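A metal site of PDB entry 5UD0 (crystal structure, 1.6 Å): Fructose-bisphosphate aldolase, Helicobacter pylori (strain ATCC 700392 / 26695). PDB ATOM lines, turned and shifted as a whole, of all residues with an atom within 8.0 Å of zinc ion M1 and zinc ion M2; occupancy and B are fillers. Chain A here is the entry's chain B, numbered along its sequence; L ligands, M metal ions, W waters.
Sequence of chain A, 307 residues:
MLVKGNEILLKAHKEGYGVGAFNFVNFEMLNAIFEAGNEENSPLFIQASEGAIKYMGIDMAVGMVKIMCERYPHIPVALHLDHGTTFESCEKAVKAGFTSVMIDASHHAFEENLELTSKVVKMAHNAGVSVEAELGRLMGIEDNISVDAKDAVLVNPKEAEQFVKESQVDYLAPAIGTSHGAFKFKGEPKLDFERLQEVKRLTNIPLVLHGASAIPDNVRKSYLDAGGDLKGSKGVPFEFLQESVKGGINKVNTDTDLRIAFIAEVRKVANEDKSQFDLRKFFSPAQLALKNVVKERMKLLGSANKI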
ATOM      1  N   ASN A  23     -20.621  -7.917 -13.051  1.00  0.00           N
ATOM      2  CA  ASN A  23     -21.577  -8.302 -14.083  1.00  0.00           C
ATOM      3  C   ASN A  23     -22.865  -7.516 -13.947  1.00  0.00           C
ATOM      4  O   ASN A  23     -23.261  -7.120 -12.834  1.00  0.00           O
ATOM      5  CB  ASN A  23     -21.879  -9.780 -13.989  1.00  0.00           C
ATOM      6  CG  ASN A  23     -20.742 -10.631 -14.523  1.00  0.00           C
ATOM      7  OD1 ASN A  23     -19.762 -10.861 -13.833  1.00  0.00           O
ATOM      8  ND2 ASN A  23     -20.897 -11.119 -15.737  1.00  0.00           N
ATOM      9  N   GLN A  47     -19.013  -5.882 -16.848  1.00  0.00           N
ATOM     10  CA  GLN A  47     -18.962  -6.988 -17.784  1.00  0.00           C
ATOM     11  C   GLN A  47     -20.341  -7.607 -17.962  1.00  0.00           C
ATOM     12  O   GLN A  47     -21.233  -7.491 -17.105  1.00  0.00           O
ATOM     13  CB  GLN A  47     -17.900  -8.036 -17.390  1.00  0.00           C
ATOM     14  CG  GLN A  47     -17.936  -8.576 -16.000  1.00  0.00           C
ATOM     15  CD  GLN A  47     -16.832  -9.620 -15.745  1.00  0.00           C
ATOM     16  OE1 GLN A  47     -15.719  -9.556 -16.268  1.00  0.00           O
ATOM     17  NE2 GLN A  47     -17.157 -10.616 -14.919  1.00  0.00           N
ATOM     18  N   ASP A  82     -17.813 -11.065 -20.946  1.00  0.00           N
ATOM     19  CA  ASP A  82     -17.493 -12.112 -19.990  1.00  0.00           C
ATOM     20  C   ASP A  82     -17.760 -13.474 -20.618  1.00  0.00           C
ATOM     21  O   ASP A  82     -18.850 -13.736 -21.126  1.00  0.00           O
ATOM     22  CB  ASP A  82     -18.333 -11.901 -18.731  1.00  0.00           C
ATOM     23  CG  ASP A  82     -17.986 -12.840 -17.616  1.00  0.00           C
ATOM     24  OD1 ASP A  82     -16.825 -13.299 -17.502  1.00  0.00           O
ATOM     25  OD2 ASP A  82     -18.907 -13.075 -16.799  1.00  0.00           O
ATOM     26  N   HIS A  83     -16.746 -14.361 -20.577  1.00  0.00           N
ATOM     27  CA  HIS A  83     -16.853 -15.732 -21.085  1.00  0.00           C
ATOM     28  C   HIS A  83     -17.432 -15.781 -22.497  1.00  0.00           C
ATOM     29  O   HIS A  83     -18.438 -16.431 -22.779  1.00  0.00           O
ATOM     30  CB  HIS A  83     -17.678 -16.592 -20.134  1.00  0.00           C
ATOM     31  CG  HIS A  83     -16.894 -17.105 -18.981  1.00  0.00           C
ATOM     32  ND1 HIS A  83     -16.109 -18.223 -19.080  1.00  0.00           N
ATOM     33  CD2 HIS A  83     -16.754 -16.649 -17.718  1.00  0.00           C
ATOM     34  CE1 HIS A  83     -15.507 -18.442 -17.922  1.00  0.00           C
ATOM     35  NE2 HIS A  83     -15.871 -17.506 -17.085  1.00  0.00           N
ATOM     36  N   MET A 102     -13.273 -11.322 -23.343  1.00  0.00           N
ATOM     37  CA  MET A 102     -12.691 -12.576 -22.924  1.00  0.00           C
ATOM     38  C   MET A 102     -13.105 -13.669 -23.897  1.00  0.00           C
ATOM     39  O   MET A 102     -14.303 -13.817 -24.171  1.00  0.00           O
ATOM     40  CB  MET A 102     -13.155 -12.966 -21.539  1.00  0.00           C
ATOM     41  CG  MET A 102     -12.415 -14.187 -21.067  1.00  0.00           C
ATOM     42  SD  MET A 102     -13.462 -15.240 -20.095  1.00  0.00           S
ATOM     43  CE  MET A 102     -12.232 -16.395 -19.469  1.00  0.00           C
ATOM     44  N   ASP A 104     -12.926 -17.683 -23.875  1.00  0.00           N
ATOM     45  CA  ASP A 104     -12.713 -18.789 -22.946  1.00  0.00           C
ATOM     46  C   ASP A 104     -12.650 -20.061 -23.766  1.00  0.00           C
ATOM     47  O   ASP A 104     -13.680 -20.604 -24.177  1.00  0.00           O
ATOM     48  CB  ASP A 104     -13.799 -18.883 -21.880  1.00  0.00           C
ATOM     49  CG  ASP A 104     -13.577 -20.087 -20.938  1.00  0.00           C
ATOM     50  OD1 ASP A 104     -12.501 -20.728 -21.005  1.00  0.00           O
ATOM     51  OD2 ASP A 104     -14.487 -20.397 -20.130  1.00  0.00           O
ATOM     52  N   SER A 106     -10.527 -22.526 -22.418  1.00  0.00           N
ATOM     53  CA  SER A 106      -9.712 -23.244 -21.436  1.00  0.00           C
ATOM     54  C   SER A 106     -10.060 -24.718 -21.339  1.00  0.00           C
ATOM     55  O   SER A 106      -9.292 -25.485 -20.763  1.00  0.00           O
ATOM     56  CB  SER A 106      -9.844 -22.613 -20.047  1.00  0.00           C
ATOM     57  OG  SER A 106     -11.102 -22.894 -19.473  1.00  0.00           O
ATOM     58  N   GLU A 132      -8.847 -10.901 -22.831  1.00  0.00           N
ATOM     59  CA  GLU A 132      -8.616 -11.841 -21.746  1.00  0.00           C
ATOM     60  C   GLU A 132      -8.761 -13.271 -22.254  1.00  0.00           C
ATOM     61  O   GLU A 132      -9.647 -13.565 -23.058  1.00  0.00           O
ATOM     62  CB  GLU A 132      -9.624 -11.615 -20.606  1.00  0.00           C
ATOM     63  CG  GLU A 132      -9.511 -12.571 -19.409  1.00  0.00           C
ATOM     64  CD  GLU A 132     -10.620 -12.339 -18.398  1.00  0.00           C
ATOM     65  OE1 GLU A 132     -11.018 -11.166 -18.145  1.00  0.00           O
ATOM     66  OE2 GLU A 132     -11.077 -13.337 -17.795  1.00  0.00           O
ATOM     67  N   GLU A 134      -8.163 -17.637 -20.626  1.00  0.00           N
ATOM     68  CA  GLU A 134      -8.221 -18.449 -19.421  1.00  0.00           C
ATOM     69  C   GLU A 134      -7.440 -19.742 -19.631  1.00  0.00           C
ATOM     70  O   GLU A 134      -7.522 -20.368 -20.683  1.00  0.00           O
ATOM     71  CB  GLU A 134      -9.650 -18.790 -19.056  1.00  0.00           C
ATOM     72  CG  GLU A 134      -9.814 -19.568 -17.776  1.00  0.00           C
ATOM     73  CD  GLU A 134     -11.258 -19.638 -17.320  1.00  0.00           C
ATOM     74  OE1 GLU A 134     -12.121 -20.063 -18.130  1.00  0.00           O
ATOM     75  OE2 GLU A 134     -11.551 -19.283 -16.176  1.00  0.00           O
ATOM     76  N   ALA A 173      -6.606 -15.220 -17.033  1.00  0.00           N
ATOM     77  CA  ALA A 173      -7.302 -15.791 -15.889  1.00  0.00           C
ATOM     78  C   ALA A 173      -6.695 -17.162 -15.633  1.00  0.00           C
ATOM     79  O   ALA A 173      -7.050 -18.132 -16.317  1.00  0.00           O
ATOM     80  CB  ALA A 173      -8.804 -15.928 -16.159  1.00  0.00           C
ATOM     81  N   THR A 178     -10.644 -21.383  -7.689  1.00  0.00           N
ATOM     82  CA  THR A 178     -11.989 -20.838  -7.580  1.00  0.00           C
ATOM     83  C   THR A 178     -12.921 -21.498  -8.588  1.00  0.00           C
ATOM     84  O   THR A 178     -12.506 -22.283  -9.443  1.00  0.00           O
ATOM     85  CB  THR A 178     -12.012 -19.338  -7.842  1.00  0.00           C
ATOM     86  OG1 THR A 178     -11.445 -19.088  -9.134  1.00  0.00           O
ATOM     87  CG2 THR A 178     -11.225 -18.593  -6.758  1.00  0.00           C
ATOM     88  N   SER A 179     -14.200 -21.147  -8.477  1.00  0.00           N
ATOM     89  CA  SER A 179     -15.221 -21.582  -9.418  1.00  0.00           C
ATOM     90  C   SER A 179     -16.381 -20.601  -9.319  1.00  0.00           C
ATOM     91  O   SER A 179     -16.540 -19.912  -8.310  1.00  0.00           O
ATOM     92  CB  SER A 179     -15.681 -23.007  -9.098  1.00  0.00           C
ATOM     93  OG  SER A 179     -16.044 -23.076  -7.737  1.00  0.00           O
ATOM     94  N   HIS A 180     -17.183 -20.546 -10.377  1.00  0.00           N
ATOM     95  CA  HIS A 180     -18.335 -19.646 -10.379  1.00  0.00           C
ATOM     96  C   HIS A 180     -19.377 -20.089  -9.361  1.00  0.00           C
ATOM     97  O   HIS A 180     -19.528 -21.276  -9.059  1.00  0.00           O
ATOM     98  CB  HIS A 180     -19.007 -19.610 -11.753  1.00  0.00           C
ATOM     99  CG  HIS A 180     -18.160 -19.035 -12.828  1.00  0.00           C
ATOM    100  ND1 HIS A 180     -18.663 -18.694 -14.071  1.00  0.00           N
ATOM    101  CD2 HIS A 180     -16.836 -18.742 -12.857  1.00  0.00           C
ATOM    102  CE1 HIS A 180     -17.684 -18.210 -14.812  1.00  0.00           C
ATOM    103  NE2 HIS A 180     -16.567 -18.225 -14.108  1.00  0.00           N
ATOM    104  N   GLY A 181     -20.161 -19.128  -8.891  1.00  0.00           N
ATOM    105  CA  GLY A 181     -21.354 -19.459  -8.119  1.00  0.00           C
ATOM    106  C   GLY A 181     -21.106 -19.465  -6.629  1.00  0.00           C
ATOM    107  O   GLY A 181     -20.022 -19.176  -6.130  1.00  0.00           O
ATOM    108  N   VAL A 208      -6.418 -12.286 -13.820  1.00  0.00           N
ATOM    109  CA  VAL A 208      -7.841 -12.262 -13.546  1.00  0.00           C
ATOM    110  C   VAL A 208      -8.240 -13.437 -12.653  1.00  0.00           C
ATOM    111  O   VAL A 208      -7.877 -14.588 -12.910  1.00  0.00           O
ATOM    112  CB  VAL A 208      -8.661 -12.298 -14.857  1.00  0.00           C
ATOM    113  CG1 VAL A 208     -10.116 -12.085 -14.595  1.00  0.00           C
ATOM    114  CG2 VAL A 208      -8.103 -11.268 -15.865  1.00  0.00           C
ATOM    115  N   LEU A 209      -9.065 -13.137 -11.666  1.00  0.00           N
ATOM    116  CA  LEU A 209      -9.618 -14.121 -10.759  1.00  0.00           C
ATOM    117  C   LEU A 209     -11.090 -14.261 -11.098  1.00  0.00           C
ATOM    118  O   LEU A 209     -11.881 -13.324 -10.918  1.00  0.00           O
ATOM    119  CB  LEU A 209      -9.456 -13.744  -9.291  1.00  0.00           C
ATOM    120  CG  LEU A 209      -9.893 -14.878  -8.360  1.00  0.00           C
ATOM    121  CD1 LEU A 209      -8.925 -16.064  -8.455  1.00  0.00           C
ATOM    122  CD2 LEU A 209      -9.982 -14.342  -6.933  1.00  0.00           C
ATOM    123  N   HIS A 210     -11.436 -15.429 -11.607  1.00  0.00           N
ATOM    124  CA  HIS A 210     -12.819 -15.778 -11.813  1.00  0.00           C
ATOM    125  C   HIS A 210     -13.367 -16.434 -10.562  1.00  0.00           C
ATOM    126  O   HIS A 210     -12.610 -16.974  -9.757  1.00  0.00           O
ATOM    127  CB  HIS A 210     -12.956 -16.739 -13.007  1.00  0.00           C
ATOM    128  CG  HIS A 210     -12.827 -16.057 -14.313  1.00  0.00           C
ATOM    129  ND1 HIS A 210     -13.830 -16.057 -15.270  1.00  0.00           N
ATOM    130  CD2 HIS A 210     -11.843 -15.280 -14.821  1.00  0.00           C
ATOM    131  CE1 HIS A 210     -13.443 -15.355 -16.316  1.00  0.00           C
ATOM    132  NE2 HIS A 210     -12.235 -14.860 -16.059  1.00  0.00           N
ATOM    133  N   GLY A 211     -14.684 -16.403 -10.443  1.00  0.00           N
ATOM    134  CA  GLY A 211     -15.377 -17.010  -9.326  1.00  0.00           C
ATOM    135  C   GLY A 211     -14.971 -16.372  -8.010  1.00  0.00           C
ATOM    136  O   GLY A 211     -14.702 -17.068  -7.035  1.00  0.00           O
ATOM    137  N   ALA A 212     -14.893 -15.035  -7.971  1.00  0.00           N
ATOM    138  CA  ALA A 212     -14.323 -14.335  -6.815  1.00  0.00           C
ATOM    139  C   ALA A 212     -15.366 -13.768  -5.853  1.00  0.00           C
ATOM    140  O   ALA A 212     -15.009 -12.934  -5.006  1.00  0.00           O
ATOM    141  CB  ALA A 212     -13.405 -13.213  -7.304  1.00  0.00           C
ATOM    142  N   LYS A 251      -7.869  -8.057 -11.898  1.00  0.00           N
ATOM    143  CA  LYS A 251      -9.283  -8.042 -12.290  1.00  0.00           C
ATOM    144  C   LYS A 251      -9.983  -9.126 -11.495  1.00  0.00           C
ATOM    145  O   LYS A 251      -9.538 -10.269 -11.469  1.00  0.00           O
ATOM    146  CB  LYS A 251      -9.439  -8.288 -13.808  1.00  0.00           C
ATOM    147  CG  LYS A 251     -10.896  -8.339 -14.307  1.00  0.00           C
ATOM    148  CD  LYS A 251     -10.945  -8.510 -15.814  1.00  0.00           C
ATOM    149  CE  LYS A 251     -12.374  -8.713 -16.373  1.00  0.00           C
ATOM    150  NZ  LYS A 251     -12.797 -10.113 -16.349  1.00  0.00           N
ATOM    151  N   ASN A 253     -13.549 -10.908 -10.851  1.00  0.00           N
ATOM    152  CA  ASN A 253     -14.881 -11.089 -11.390  1.00  0.00           C
ATOM    153  C   ASN A 253     -15.894 -11.339 -10.274  1.00  0.00           C
ATOM    154  O   ASN A 253     -15.729 -12.264  -9.472  1.00  0.00           O
ATOM    155  CB  ASN A 253     -14.918 -12.265 -12.379  1.00  0.00           C
ATOM    156  CG  ASN A 253     -14.185 -11.979 -13.667  1.00  0.00           C
ATOM    157  OD1 ASN A 253     -13.321 -11.106 -13.721  1.00  0.00           O
ATOM    158  ND2 ASN A 253     -14.565 -12.699 -14.722  1.00  0.00           N
ATOM    159  N   THR A 254     -16.977 -10.551 -10.265  1.00  0.00           N
ATOM    160  CA  THR A 254     -17.937 -10.558  -9.180  1.00  0.00           C
ATOM    161  C   THR A 254     -19.342 -10.424  -9.727  1.00  0.00           C
ATOM    162  O   THR A 254     -19.672  -9.435 -10.382  1.00  0.00           O
ATOM    163  CB  THR A 254     -17.666  -9.407  -8.192  1.00  0.00           C
ATOM    164  OG1 THR A 254     -16.274  -9.358  -7.876  1.00  0.00           O
ATOM    165  CG2 THR A 254     -18.458  -9.605  -6.942  1.00  0.00           C
ATOM    166  N   ASP A 255     -20.182 -11.395  -9.382  1.00  0.00           N
ATOM    167  CA  ASP A 255     -21.541 -11.484  -9.906  1.00  0.00           C
ATOM    168  C   ASP A 255     -22.481 -12.041  -8.846  1.00  0.00           C
ATOM    169  O   ASP A 255     -23.469 -11.397  -8.481  1.00  0.00           O
ATOM    170  CB  ASP A 255     -21.523 -12.344 -11.165  1.00  0.00           C
ATOM    171  CG  ASP A 255     -22.852 -12.352 -11.919  1.00  0.00           C
ATOM    172  OD1 ASP A 255     -23.845 -11.770 -11.436  1.00  0.00           O
ATOM    173  OD2 ASP A 255     -22.899 -12.901 -13.057  1.00  0.00           O
HETATM  174  P1  LIG L   1     -18.925 -15.342  -8.899  1.00  0.00           P
HETATM  175  O1  LIG L   1     -17.976 -15.794  -7.808  1.00  0.00           O
HETATM  176  O2  LIG L   1     -19.974 -16.319  -9.394  1.00  0.00           O
HETATM  177  O3  LIG L   1     -19.501 -13.955  -8.700  1.00  0.00           O
HETATM  178  O4  LIG L   1     -17.892 -15.215 -10.156  1.00  0.00           O
HETATM  179  C1  LIG L   1     -18.142 -14.297 -11.198  1.00  0.00           C
HETATM  180  C2  LIG L   1     -17.279 -14.539 -12.412  1.00  0.00           C
HETATM  181  O5  LIG L   1     -16.377 -15.354 -12.455  1.00  0.00           O
HETATM  182  C3  LIG L   1     -17.882 -14.202 -13.733  1.00  0.00           C
HETATM  183  O6  LIG L   1     -16.923 -14.135 -14.786  1.00  0.00           O
HETATM  184 ZN    ZN M   1     -15.189 -17.639 -15.399  1.00  0.00          ZN
HETATM  185 ZN    ZN M   2     -16.107 -16.382 -14.807  1.00  0.00          ZN
HETATM  186 CA    CA M   3     -13.170 -21.807 -19.072  1.00  0.00          CA
HETATM  187  O   HOH W   1     -13.741 -19.059 -15.794  1.00  0.00           O
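An oxygen (O2) of the ligand sits at hydrogen-bond distance from the backbone NH (N) of Gly 181.
ND2 of Asn 253 sits close to O6 of the ligand.
N of Asp 255 sits at hydrogen-bond distance from O3 of the ligand (2.7 Å).
The side-chain carboxylate (OD1) of Asp 82 sits close to an oxygen (O6) of the ligand (2.8 Å).
An oxygen (O1) of the ligand sits at hydrogen-bond distance from the backbone NH (N) of Ala 212.
An oxygen (O4) of the ligand sits close to the backbone NH (N) of Gly 211 (3.4 Å).
A ring nitrogen (NE2) of His 210 sits at hydrogen-bond distance from the side-chain carboxylate (OE2) of Glu 132 (2.6 Å).
O of Leu 209 lies within hydrogen-bond range of N of Asn 253 (2.9 Å).
OD1 of Asn 253 sits at hydrogen-bond distance from NZ of Lys 251 (2.9 Å).
The side-chain amide nitrogen (ND2) of Asn 253 lies close to the side-chain amide nitrogen (NE2) of Gln 47 (3.3 Å).
The backbone carbonyl oxygen (O) of His 210 lies within hydrogen-bond range of the side-chain hydroxyl (OG1) of Thr 178 (2.5 Å).
The side-chain amide nitrogen (ND2) of Asn 253 lies close to a ring nitrogen (NE2) of His 210.
The backbone carbonyl oxygen of Asn 253 lies within hydrogen-bond range of the backbone NH of Ala 212 (3.3 Å).
A ring nitrogen (ND1) of His 83 sits close to the side-chain carboxylate of Asp 104, 2.9 Å away.
Within 4 Å of zinc ion M1: His 83, His 180 and His 210.
ND2 of Asn 253 touches zinc ion M2 (3.99 Å).
The nearest printed residue that does not touch zinc ion M2 is Asp 82 (4.2 Å).
Zinc ion M1 is bound by NE2 of His 83 (1.8 Å), NE2 of His 180 (2.0 Å), water W1 (2.1 Å) and ND1 of His 210 (2.1 Å).
Zinc ion M2 is bound by NE2 of His 180 (2.0 Å).
ND1 of His 210 is bound to zinc ion M2.
An oxygen (O6) of the ligand binds zinc ion M2, at 2.4 Å.
Zinc ion M2 is bound by NE2 of His 83.
Zinc ion M2 is bound by O5 of the ligand (2.6 Å).
Zinc ion M2 has five donor atoms within binding distance.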
